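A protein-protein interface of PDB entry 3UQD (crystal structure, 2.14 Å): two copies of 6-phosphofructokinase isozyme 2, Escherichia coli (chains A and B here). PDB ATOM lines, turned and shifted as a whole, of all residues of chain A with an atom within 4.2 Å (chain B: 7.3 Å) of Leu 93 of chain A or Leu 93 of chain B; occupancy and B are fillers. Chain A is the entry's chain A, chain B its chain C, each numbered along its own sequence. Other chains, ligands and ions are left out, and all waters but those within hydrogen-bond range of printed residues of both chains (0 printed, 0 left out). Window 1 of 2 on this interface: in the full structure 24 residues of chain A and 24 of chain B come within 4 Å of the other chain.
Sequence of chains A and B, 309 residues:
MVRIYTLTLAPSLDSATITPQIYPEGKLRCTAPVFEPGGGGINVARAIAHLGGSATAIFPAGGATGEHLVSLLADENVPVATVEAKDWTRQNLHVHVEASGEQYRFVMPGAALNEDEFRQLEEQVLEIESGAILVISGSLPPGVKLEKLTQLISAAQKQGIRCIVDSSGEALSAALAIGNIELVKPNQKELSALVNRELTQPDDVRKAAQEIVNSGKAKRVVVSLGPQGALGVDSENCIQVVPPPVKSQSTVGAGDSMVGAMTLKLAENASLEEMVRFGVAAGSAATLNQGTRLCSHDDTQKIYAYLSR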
ATOM      1  N   SER A  15     -11.388   5.947  -9.084  1.00  0.00           N
ATOM      2  CA  SER A  15     -12.361   4.947  -9.484  1.00  0.00           C
ATOM      3  C   SER A  15     -12.710   5.102 -10.965  1.00  0.00           C
ATOM      4  O   SER A  15     -12.852   6.215 -11.472  1.00  0.00           O
ATOM      5  CB  SER A  15     -13.614   5.043  -8.621  1.00  0.00           C
ATOM      6  OG  SER A  15     -14.201   6.321  -8.752  1.00  0.00           O
ATOM      7  N   THR A  17     -15.318   3.802 -14.111  1.00  0.00           N
ATOM      8  CA  THR A  17     -16.587   3.163 -14.438  1.00  0.00           C
ATOM      9  C   THR A  17     -16.881   3.240 -15.937  1.00  0.00           C
ATOM     10  O   THR A  17     -16.267   4.028 -16.657  1.00  0.00           O
ATOM     11  CB  THR A  17     -17.750   3.795 -13.657  1.00  0.00           C
ATOM     12  OG1 THR A  17     -18.966   3.104 -13.963  1.00  0.00           O
ATOM     13  CG2 THR A  17     -17.910   5.258 -14.023  1.00  0.00           C
ATOM     14  N   ASN A  92     -11.443  10.293  -7.119  1.00  0.00           N
ATOM     15  CA  ASN A  92     -11.741  10.803  -8.459  1.00  0.00           C
ATOM     16  C   ASN A  92     -12.524   9.792  -9.297  1.00  0.00           C
ATOM     17  O   ASN A  92     -12.493   8.595  -9.017  1.00  0.00           O
ATOM     18  CB  ASN A  92     -10.447  11.203  -9.172  1.00  0.00           C
ATOM     19  CG  ASN A  92      -9.717  12.339  -8.459  1.00  0.00           C
ATOM     20  OD1 ASN A  92     -10.323  13.118  -7.725  1.00  0.00           O
ATOM     21  ND2 ASN A  92      -8.413  12.440  -8.682  1.00  0.00           N
ATOM     22  N   LEU A  93     -13.231  10.267 -10.321  1.00  0.00           N
ATOM     23  CA  LEU A  93     -14.019   9.373 -11.169  1.00  0.00           C
ATOM     24  C   LEU A  93     -13.638   9.463 -12.645  1.00  0.00           C
ATOM     25  O   LEU A  93     -13.676  10.535 -13.246  1.00  0.00           O
ATOM     26  CB  LEU A  93     -15.519   9.639 -11.004  1.00  0.00           C
ATOM     27  CG  LEU A  93     -16.449   8.698 -11.780  1.00  0.00           C
ATOM     28  CD1 LEU A  93     -16.330   7.275 -11.254  1.00  0.00           C
ATOM     29  CD2 LEU A  93     -17.892   9.178 -11.709  1.00  0.00           C
ATOM     30  N   HIS A  94     -13.292   8.318 -13.221  1.00  0.00           N
ATOM     31  CA  HIS A  94     -12.943   8.218 -14.634  1.00  0.00           C
ATOM     32  C   HIS A  94     -14.065   7.479 -15.363  1.00  0.00           C
ATOM     33  O   HIS A  94     -14.385   6.342 -15.028  1.00  0.00           O
ATOM     34  CB  HIS A  94     -11.610   7.471 -14.786  1.00  0.00           C
ATOM     35  CG  HIS A  94     -11.200   7.236 -16.208  1.00  0.00           C
ATOM     36  ND1 HIS A  94     -11.666   6.174 -16.952  1.00  0.00           N
ATOM     37  CD2 HIS A  94     -10.355   7.919 -17.018  1.00  0.00           C
ATOM     38  CE1 HIS A  94     -11.134   6.217 -18.161  1.00  0.00           C
ATOM     39  NE2 HIS A  94     -10.334   7.265 -18.226  1.00  0.00           N
ATOM     40  N   VAL A  95     -14.670   8.123 -16.353  1.00  0.00           N
ATOM     41  CA  VAL A  95     -15.827   7.545 -17.032  1.00  0.00           C
ATOM     42  C   VAL A  95     -15.569   7.281 -18.519  1.00  0.00           C
ATOM     43  O   VAL A  95     -15.267   8.198 -19.273  1.00  0.00           O
ATOM     44  CB  VAL A  95     -17.069   8.451 -16.884  1.00  0.00           C
ATOM     45  CG1 VAL A  95     -18.271   7.838 -17.590  1.00  0.00           C
ATOM     46  CG2 VAL A  95     -17.380   8.680 -15.413  1.00  0.00           C
ATOM     47  N   TYR A 104     -13.911  10.549 -19.635  1.00  0.00           N
ATOM     48  CA  TYR A 104     -14.138  11.780 -18.880  1.00  0.00           C
ATOM     49  C   TYR A 104     -13.540  11.673 -17.488  1.00  0.00           C
ATOM     50  O   TYR A 104     -13.748  10.683 -16.789  1.00  0.00           O
ATOM     51  CB  TYR A 104     -15.641  12.097 -18.801  1.00  0.00           C
ATOM     52  CG  TYR A 104     -16.234  12.463 -20.144  1.00  0.00           C
ATOM     53  CD1 TYR A 104     -16.643  11.480 -21.035  1.00  0.00           C
ATOM     54  CD2 TYR A 104     -16.358  13.790 -20.530  1.00  0.00           C
ATOM     55  CE1 TYR A 104     -17.171  11.807 -22.270  1.00  0.00           C
ATOM     56  CE2 TYR A 104     -16.884  14.132 -21.770  1.00  0.00           C
ATOM     57  CZ  TYR A 104     -17.290  13.136 -22.635  1.00  0.00           C
ATOM     58  OH  TYR A 104     -17.812  13.465 -23.867  1.00  0.00           O
ATOM     59  N   ARG A 105     -12.798  12.701 -17.089  1.00  0.00           N
ATOM     60  CA  ARG A 105     -12.020  12.647 -15.858  1.00  0.00           C
ATOM     61  C   ARG A 105     -12.424  13.728 -14.869  1.00  0.00           C
ATOM     62  O   ARG A 105     -12.009  14.880 -14.995  1.00  0.00           O
ATOM     63  CB  ARG A 105     -10.536  12.781 -16.181  1.00  0.00           C
ATOM     64  CG  ARG A 105     -10.051  11.799 -17.221  1.00  0.00           C
ATOM     65  CD  ARG A 105      -8.749  12.266 -17.841  1.00  0.00           C
ATOM     66  NE  ARG A 105      -7.674  12.361 -16.859  1.00  0.00           N
ATOM     67  CZ  ARG A 105      -6.443  12.774 -17.142  1.00  0.00           C
ATOM     68  NH1 ARG A 105      -6.132  13.137 -18.380  1.00  0.00           N
ATOM     69  NH2 ARG A 105      -5.523  12.825 -16.189  1.00  0.00           N
ATOM     70  N   PHE A 106     -13.219  13.347 -13.876  1.00  0.00           N
ATOM     71  CA  PHE A 106     -13.687  14.287 -12.863  1.00  0.00           C
ATOM     72  C   PHE A 106     -12.733  14.324 -11.669  1.00  0.00           C
ATOM     73  O   PHE A 106     -12.641  13.368 -10.897  1.00  0.00           O
ATOM     74  CB  PHE A 106     -15.120  13.946 -12.437  1.00  0.00           C
ATOM     75  CG  PHE A 106     -16.100  13.955 -13.577  1.00  0.00           C
ATOM     76  CD1 PHE A 106     -16.691  15.142 -13.993  1.00  0.00           C
ATOM     77  CD2 PHE A 106     -16.411  12.785 -14.250  1.00  0.00           C
ATOM     78  CE1 PHE A 106     -17.584  15.158 -15.050  1.00  0.00           C
ATOM     79  CE2 PHE A 106     -17.305  12.791 -15.309  1.00  0.00           C
ATOM     80  CZ  PHE A 106     -17.892  13.981 -15.711  1.00  0.00           C
ATOM     81  N   MET A 108     -11.522  15.776  -8.186  1.00  0.00           N
ATOM     82  CA  MET A 108     -11.894  16.431  -6.933  1.00  0.00           C
ATOM     83  C   MET A 108     -10.686  17.112  -6.289  1.00  0.00           C
ATOM     84  O   MET A 108      -9.546  16.796  -6.625  1.00  0.00           O
ATOM     85  CB  MET A 108     -12.472  15.393  -5.967  1.00  0.00           C
ATOM     86  CG  MET A 108     -13.516  14.496  -6.593  1.00  0.00           C
ATOM     87  SD  MET A 108     -14.964  15.418  -7.114  1.00  0.00           S
ATOM     88  CE  MET A 108     -15.401  14.522  -8.600  1.00  0.00           C
ATOM     89  N   SER B  12     -28.585   5.138  -1.768  1.00  0.00           N
ATOM     90  CA  SER B  12     -27.416   5.790  -2.335  1.00  0.00           C
ATOM     91  C   SER B  12     -26.972   6.978  -1.500  1.00  0.00           C
ATOM     92  O   SER B  12     -27.783   7.807  -1.101  1.00  0.00           O
ATOM     93  CB  SER B  12     -27.694   6.254  -3.767  1.00  0.00           C
ATOM     94  OG  SER B  12     -26.646   7.087  -4.238  1.00  0.00           O
ATOM     95  N   LEU B  13     -25.679   7.048  -1.225  1.00  0.00           N
ATOM     96  CA  LEU B  13     -25.094   8.277  -0.729  1.00  0.00           C
ATOM     97  C   LEU B  13     -24.837   9.153  -1.946  1.00  0.00           C
ATOM     98  O   LEU B  13     -23.886   8.927  -2.694  1.00  0.00           O
ATOM     99  CB  LEU B  13     -23.788   8.007   0.017  1.00  0.00           C
ATOM    100  CG  LEU B  13     -23.144   9.242   0.649  1.00  0.00           C
ATOM    101  CD1 LEU B  13     -23.995   9.761   1.805  1.00  0.00           C
ATOM    102  CD2 LEU B  13     -21.720   8.947   1.100  1.00  0.00           C
ATOM    103  N   ASP B  14     -25.713  10.132  -2.152  1.00  0.00           N
ATOM    104  CA  ASP B  14     -25.610  11.052  -3.279  1.00  0.00           C
ATOM    105  C   ASP B  14     -24.512  12.085  -3.049  1.00  0.00           C
ATOM    106  O   ASP B  14     -24.405  12.662  -1.967  1.00  0.00           O
ATOM    107  CB  ASP B  14     -26.942  11.773  -3.497  1.00  0.00           C
ATOM    108  CG  ASP B  14     -27.947  10.939  -4.265  1.00  0.00           C
ATOM    109  OD1 ASP B  14     -27.651   9.764  -4.575  1.00  0.00           O
ATOM    110  OD2 ASP B  14     -29.044  11.464  -4.559  1.00  0.00           O
ATOM    111  N   SER B  15     -23.705  12.318  -4.076  1.00  0.00           N
ATOM    112  CA  SER B  15     -22.680  13.352  -4.022  1.00  0.00           C
ATOM    113  C   SER B  15     -22.864  14.344  -5.172  1.00  0.00           C
ATOM    114  O   SER B  15     -23.067  13.953  -6.323  1.00  0.00           O
ATOM    115  CB  SER B  15     -21.282  12.731  -4.057  1.00  0.00           C
ATOM    116  OG  SER B  15     -21.125  11.903  -5.196  1.00  0.00           O
ATOM    117  N   ALA B  16     -22.807  15.632  -4.849  1.00  0.00           N
ATOM    118  CA  ALA B  16     -23.000  16.678  -5.846  1.00  0.00           C
ATOM    119  C   ALA B  16     -21.771  17.570  -5.936  1.00  0.00           C
ATOM    120  O   ALA B  16     -21.228  17.993  -4.916  1.00  0.00           O
ATOM    121  CB  ALA B  16     -24.232  17.504  -5.519  1.00  0.00           C
ATOM    122  N   THR B  17     -21.337  17.847  -7.163  1.00  0.00           N
ATOM    123  CA  THR B  17     -20.185  18.712  -7.402  1.00  0.00           C
ATOM    124  C   THR B  17     -20.456  19.680  -8.557  1.00  0.00           C
ATOM    125  O   THR B  17     -21.423  19.518  -9.302  1.00  0.00           O
ATOM    126  CB  THR B  17     -18.915  17.887  -7.700  1.00  0.00           C
ATOM    127  OG1 THR B  17     -17.767  18.743  -7.691  1.00  0.00           O
ATOM    128  CG2 THR B  17     -19.029  17.191  -9.052  1.00  0.00           C
ATOM    129  N   CYS B  30     -13.339  19.740 -10.316  1.00  0.00           N
ATOM    130  CA  CYS B  30     -14.631  19.804  -9.658  1.00  0.00           C
ATOM    131  C   CYS B  30     -14.488  20.361  -8.249  1.00  0.00           C
ATOM    132  O   CYS B  30     -13.416  20.296  -7.653  1.00  0.00           O
ATOM    133  CB  CYS B  30     -15.286  18.420  -9.631  1.00  0.00           C
ATOM    134  SG  CYS B  30     -15.633  17.747 -11.273  1.00  0.00           S
ATOM    135  N   PRO B  33     -17.216  18.033  -3.089  1.00  0.00           N
ATOM    136  CA  PRO B  33     -18.539  17.411  -3.197  1.00  0.00           C
ATOM    137  C   PRO B  33     -19.384  17.586  -1.940  1.00  0.00           C
ATOM    138  O   PRO B  33     -18.855  17.606  -0.827  1.00  0.00           O
ATOM    139  CB  PRO B  33     -18.214  15.926  -3.402  1.00  0.00           C
ATOM    140  CG  PRO B  33     -16.815  15.908  -3.919  1.00  0.00           C
ATOM    141  CD  PRO B  33     -16.133  17.046  -3.234  1.00  0.00           C
ATOM    142  N   GLN B  91     -22.258   5.012  -4.188  1.00  0.00           N
ATOM    143  CA  GLN B  91     -22.003   6.440  -4.136  1.00  0.00           C
ATOM    144  C   GLN B  91     -22.165   7.027  -5.538  1.00  0.00           C
ATOM    145  O   GLN B  91     -21.321   6.809  -6.410  1.00  0.00           O
ATOM    146  CB  GLN B  91     -20.588   6.678  -3.614  1.00  0.00           C
ATOM    147  CG  GLN B  91     -20.385   7.985  -2.871  1.00  0.00           C
ATOM    148  CD  GLN B  91     -19.128   7.965  -2.017  1.00  0.00           C
ATOM    149  OE1 GLN B  91     -18.386   6.979  -2.000  1.00  0.00           O
ATOM    150  NE2 GLN B  91     -18.885   9.055  -1.299  1.00  0.00           N
ATOM    151  N   ASN B  92     -23.260   7.753  -5.755  1.00  0.00           N
ATOM    152  CA  ASN B  92     -23.544   8.340  -7.061  1.00  0.00           C
ATOM    153  C   ASN B  92     -23.015   9.762  -7.172  1.00  0.00           C
ATOM    154  O   ASN B  92     -23.046  10.521  -6.201  1.00  0.00           O
ATOM    155  CB  ASN B  92     -25.044   8.318  -7.353  1.00  0.00           C
ATOM    156  CG  ASN B  92     -25.594   6.913  -7.476  1.00  0.00           C
ATOM    157  OD1 ASN B  92     -24.858   5.965  -7.762  1.00  0.00           O
ATOM    158  ND2 ASN B  92     -26.898   6.771  -7.265  1.00  0.00           N
ATOM    159  N   LEU B  93     -22.534  10.120  -8.359  1.00  0.00           N
ATOM    160  CA  LEU B  93     -21.951  11.441  -8.587  1.00  0.00           C
ATOM    161  C   LEU B  93     -22.799  12.315  -9.504  1.00  0.00           C
ATOM    162  O   LEU B  93     -23.109  11.931 -10.636  1.00  0.00           O
ATOM    163  CB  LEU B  93     -20.550  11.314  -9.181  1.00  0.00           C
ATOM    164  CG  LEU B  93     -19.838  12.656  -9.317  1.00  0.00           C
ATOM    165  CD1 LEU B  93     -19.559  13.215  -7.928  1.00  0.00           C
ATOM    166  CD2 LEU B  93     -18.553  12.520 -10.128  1.00  0.00           C
ATOM    167  N   HIS B  94     -23.152  13.499  -9.015  1.00  0.00           N
ATOM    168  CA  HIS B  94     -23.947  14.448  -9.787  1.00  0.00           C
ATOM    169  C   HIS B  94     -23.131  15.692 -10.115  1.00  0.00           C
ATOM    170  O   HIS B  94     -22.846  16.494  -9.227  1.00  0.00           O
ATOM    171  CB  HIS B  94     -25.199  14.847  -9.004  1.00  0.00           C
ATOM    172  CG  HIS B  94     -26.145  13.715  -8.758  1.00  0.00           C
ATOM    173  ND1 HIS B  94     -27.012  13.689  -7.687  1.00  0.00           N
ATOM    174  CD2 HIS B  94     -26.364  12.571  -9.448  1.00  0.00           C
ATOM    175  CE1 HIS B  94     -27.720  12.574  -7.724  1.00  0.00           C
ATOM    176  NE2 HIS B  94     -27.347  11.879  -8.783  1.00  0.00           N
ATOM    177  N   VAL B  95     -22.764  15.850 -11.385  1.00  0.00           N
ATOM    178  CA  VAL B  95     -21.924  16.967 -11.814  1.00  0.00           C
ATOM    179  C   VAL B  95     -22.727  18.078 -12.491  1.00  0.00           C
ATOM    180  O   VAL B  95     -23.361  17.864 -13.530  1.00  0.00           O
ATOM    181  CB  VAL B  95     -20.820  16.501 -12.780  1.00  0.00           C
ATOM    182  CG1 VAL B  95     -19.930  17.668 -13.172  1.00  0.00           C
ATOM    183  CG2 VAL B  95     -19.995  15.383 -12.153  1.00  0.00           C
ATOM    184  N   GLN B 103     -27.008  19.184 -15.790  1.00  0.00           N
ATOM    185  CA  GLN B 103     -26.503  18.263 -14.788  1.00  0.00           C
ATOM    186  C   GLN B 103     -26.239  16.896 -15.405  1.00  0.00           C
ATOM    187  O   GLN B 103     -27.035  16.412 -16.208  1.00  0.00           O
ATOM    188  CB  GLN B 103     -27.509  18.133 -13.645  1.00  0.00           C
ATOM    189  CG  GLN B 103     -27.030  17.273 -12.496  1.00  0.00           C
ATOM    190  CD  GLN B 103     -28.020  17.232 -11.349  1.00  0.00           C
ATOM    191  OE1 GLN B 103     -27.631  17.177 -10.182  1.00  0.00           O
ATOM    192  NE2 GLN B 103     -29.309  17.253 -11.676  1.00  0.00           N
ATOM    193  N   TYR B 104     -25.120  16.281 -15.036  1.00  0.00           N
ATOM    194  CA  TYR B 104     -24.822  14.916 -15.459  1.00  0.00           C
ATOM    195  C   TYR B 104     -24.848  13.954 -14.275  1.00  0.00           C
ATOM    196  O   TYR B 104     -24.261  14.224 -13.226  1.00  0.00           O
ATOM    197  CB  TYR B 104     -23.476  14.850 -16.176  1.00  0.00           C
ATOM    198  CG  TYR B 104     -23.499  15.511 -17.530  1.00  0.00           C
ATOM    199  CD1 TYR B 104     -23.408  16.888 -17.648  1.00  0.00           C
ATOM    200  CD2 TYR B 104     -23.621  14.758 -18.689  1.00  0.00           C
ATOM    201  CE1 TYR B 104     -23.436  17.502 -18.882  1.00  0.00           C
ATOM    202  CE2 TYR B 104     -23.645  15.364 -19.933  1.00  0.00           C
ATOM    203  CZ  TYR B 104     -23.553  16.734 -20.022  1.00  0.00           C
ATOM    204  OH  TYR B 104     -23.577  17.348 -21.257  1.00  0.00           O
ATOM    205  N   ARG B 105     -25.530  12.828 -14.451  1.00  0.00           N
ATOM    206  CA  ARG B 105     -25.786  11.913 -13.347  1.00  0.00           C
ATOM    207  C   ARG B 105     -25.134  10.561 -13.565  1.00  0.00           C
ATOM    208  O   ARG B 105     -25.566   9.786 -14.416  1.00  0.00           O
ATOM    209  CB  ARG B 105     -27.290  11.719 -13.179  1.00  0.00           C
ATOM    210  CG  ARG B 105     -28.081  12.997 -13.299  1.00  0.00           C
ATOM    211  CD  ARG B 105     -28.640  13.410 -11.964  1.00  0.00           C
ATOM    212  NE  ARG B 105     -29.600  12.437 -11.452  1.00  0.00           N
ATOM    213  CZ  ARG B 105     -30.882  12.400 -11.803  1.00  0.00           C
ATOM    214  NH1 ARG B 105     -31.361  13.279 -12.675  1.00  0.00           N
ATOM    215  NH2 ARG B 105     -31.684  11.488 -11.280  1.00  0.00           N
ATOM    216  N   PHE B 106     -24.098  10.272 -12.786  1.00  0.00           N
ATOM    217  CA  PHE B 106     -23.426   8.984 -12.885  1.00  0.00           C
ATOM    218  C   PHE B 106     -23.891   8.068 -11.757  1.00  0.00           C
ATOM    219  O   PHE B 106     -23.580   8.289 -10.587  1.00  0.00           O
ATOM    220  CB  PHE B 106     -21.908   9.170 -12.913  1.00  0.00           C
ATOM    221  CG  PHE B 106     -21.444  10.086 -14.013  1.00  0.00           C
ATOM    222  CD1 PHE B 106     -21.203   9.597 -15.287  1.00  0.00           C
ATOM    223  CD2 PHE B 106     -21.280  11.440 -13.780  1.00  0.00           C
ATOM    224  CE1 PHE B 106     -20.798  10.439 -16.304  1.00  0.00           C
ATOM    225  CE2 PHE B 106     -20.867  12.289 -14.798  1.00  0.00           C
ATOM    226  CZ  PHE B 106     -20.627  11.786 -16.059  1.00  0.00           C
ATOM    227  N   VAL B 107     -24.647   7.042 -12.139  1.00  0.00           N
ATOM    228  CA  VAL B 107     -25.415   6.222 -11.205  1.00  0.00           C
ATOM    229  C   VAL B 107     -24.861   4.806 -11.120  1.00  0.00           C
ATOM    230  O   VAL B 107     -25.061   3.996 -12.029  1.00  0.00           O
ATOM    231  CB  VAL B 107     -26.904   6.154 -11.630  1.00  0.00           C
ATOM    232  CG1 VAL B 107     -27.732   5.423 -10.589  1.00  0.00           C
ATOM    233  CG2 VAL B 107     -27.459   7.559 -11.873  1.00  0.00           C
ATOM    234  N   MET B 108     -24.167   4.521 -10.020  1.00  0.00           N
ATOM    235  CA  MET B 108     -23.529   3.228  -9.808  1.00  0.00           C
ATOM    236  C   MET B 108     -24.574   2.167  -9.488  1.00  0.00           C
ATOM    237  O   MET B 108     -25.697   2.500  -9.111  1.00  0.00           O
ATOM    238  CB  MET B 108     -22.515   3.331  -8.661  1.00  0.00           C
ATOM    239  CG  MET B 108     -21.568   4.517  -8.779  1.00  0.00           C
ATOM    240  SD  MET B 108     -20.628   4.515 -10.319  1.00  0.00           S
ATOM    241  CE  MET B 108     -19.984   6.188 -10.311  1.00  0.00           C
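Among the printed residues, pairs that only touch across the chains: Leu 93 of chain A with Leu 93 of chain B (3.8 Å), Leu 93 of chain A with Met 108 of chain B (3.9 Å), Val 95 of chain A with Phe 106 of chain B (3.8 Å), Phe 106 of chain A with Cys 30 of chain B (3.9 Å), Phe 106 of chain A with Val 95 of chain B (3.8 Å), Phe 106 of chain A with Phe 106 of chain B (3.5 Å), Met 108 of chain A with Cys 30 of chain B (3.9 Å) and Met 108 of chain A with Pro 33 of chain B (3.7 Å).
Of the 19 printed residues of chain B, 6 touch a printed residue of chain A.
Hydrophobic or aromatic side chains of chain B that line the printed part of chain A: Pro 33, Leu 93, Val 95, Phe 106 and Met 108.
Hydrophobic or aromatic side chains of chain A within 4 Å of the printed part of chain B: Leu 93, Val 95, Phe 106 and Met 108.
Along chain A the printed residues that touch a printed residue of chain B span positions 93 to 108.
Among the printed residues, no Asp or Glu carboxylate lies within 4 Å of a Lys or Arg side-chain nitrogen of the other chain.
Leu 93 of chain A touches its own counterpart, Leu 93 of chain B.
Leu 93 of chain A touches Met 108 of chain B, but with the chains exchanged Met 108 of chain A does not touch Leu 93 of chain B (4.03 Å).
Val 95 of chain A touches Phe 106 of chain B, and with the chains exchanged Phe 106 of chain A touches Val 95 of chain B.
Phe 106 of chain B touches its own counterpart, Phe 106 of chain A.
Positions printed for both chains: 15, 17, 92, 93, 94, 95, 104, 105, 106 and 108.
Of chain B, only Leu 93 (3.8 Å) and Met 108 (3.9 Å) come within 4 Å of Leu 93 of chain A.
Leu 93 of chain B touches just one residue of chain A: Leu 93.
Printed residues of chain A within 4 Å of Val 95 of chain B: Phe 106 (3.8 Å).
Of the printed residues of chain A, Cys 30 of chain B touches Phe 106 (3.9 Å) and Met 108 (3.9 Å).
His 94 of chain A touches none of the printed residues of chain B.
His 94 of chain B touches none of the printed residues of chain A.
The nearest residue of chain B that does not touch Leu 93 of chain A is Phe 106 of chain B (4.2 Å).
OD1 of Asn 92 of chain A lies within hydrogen-bond range of N of Met 108 of chain A.
The backbone carbonyl oxygen (O) of Leu 93 of chain A is in hydrogen-bond range of the backbone NH (N) of Phe 106 of chain A.
The backbone carbonyl oxygen (O) of Val 95 of chain A lies within hydrogen-bond range of the backbone NH (N) of Tyr 104 of chain A.
The side-chain amide oxygen (OD1) of Asn 92 of chain B is in hydrogen-bond range of the backbone NH (N) of Met 108 of chain B.
The backbone NH (N) of Phe 106 of chain B is in hydrogen-bond range of the backbone carbonyl oxygen (O) of Leu 93 of chain B (2.9 Å).
The backbone carbonyl oxygen of Val 95 of chain B is in hydrogen-bond range of the backbone NH of Tyr 104 of chain B, at 2.8 Å.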
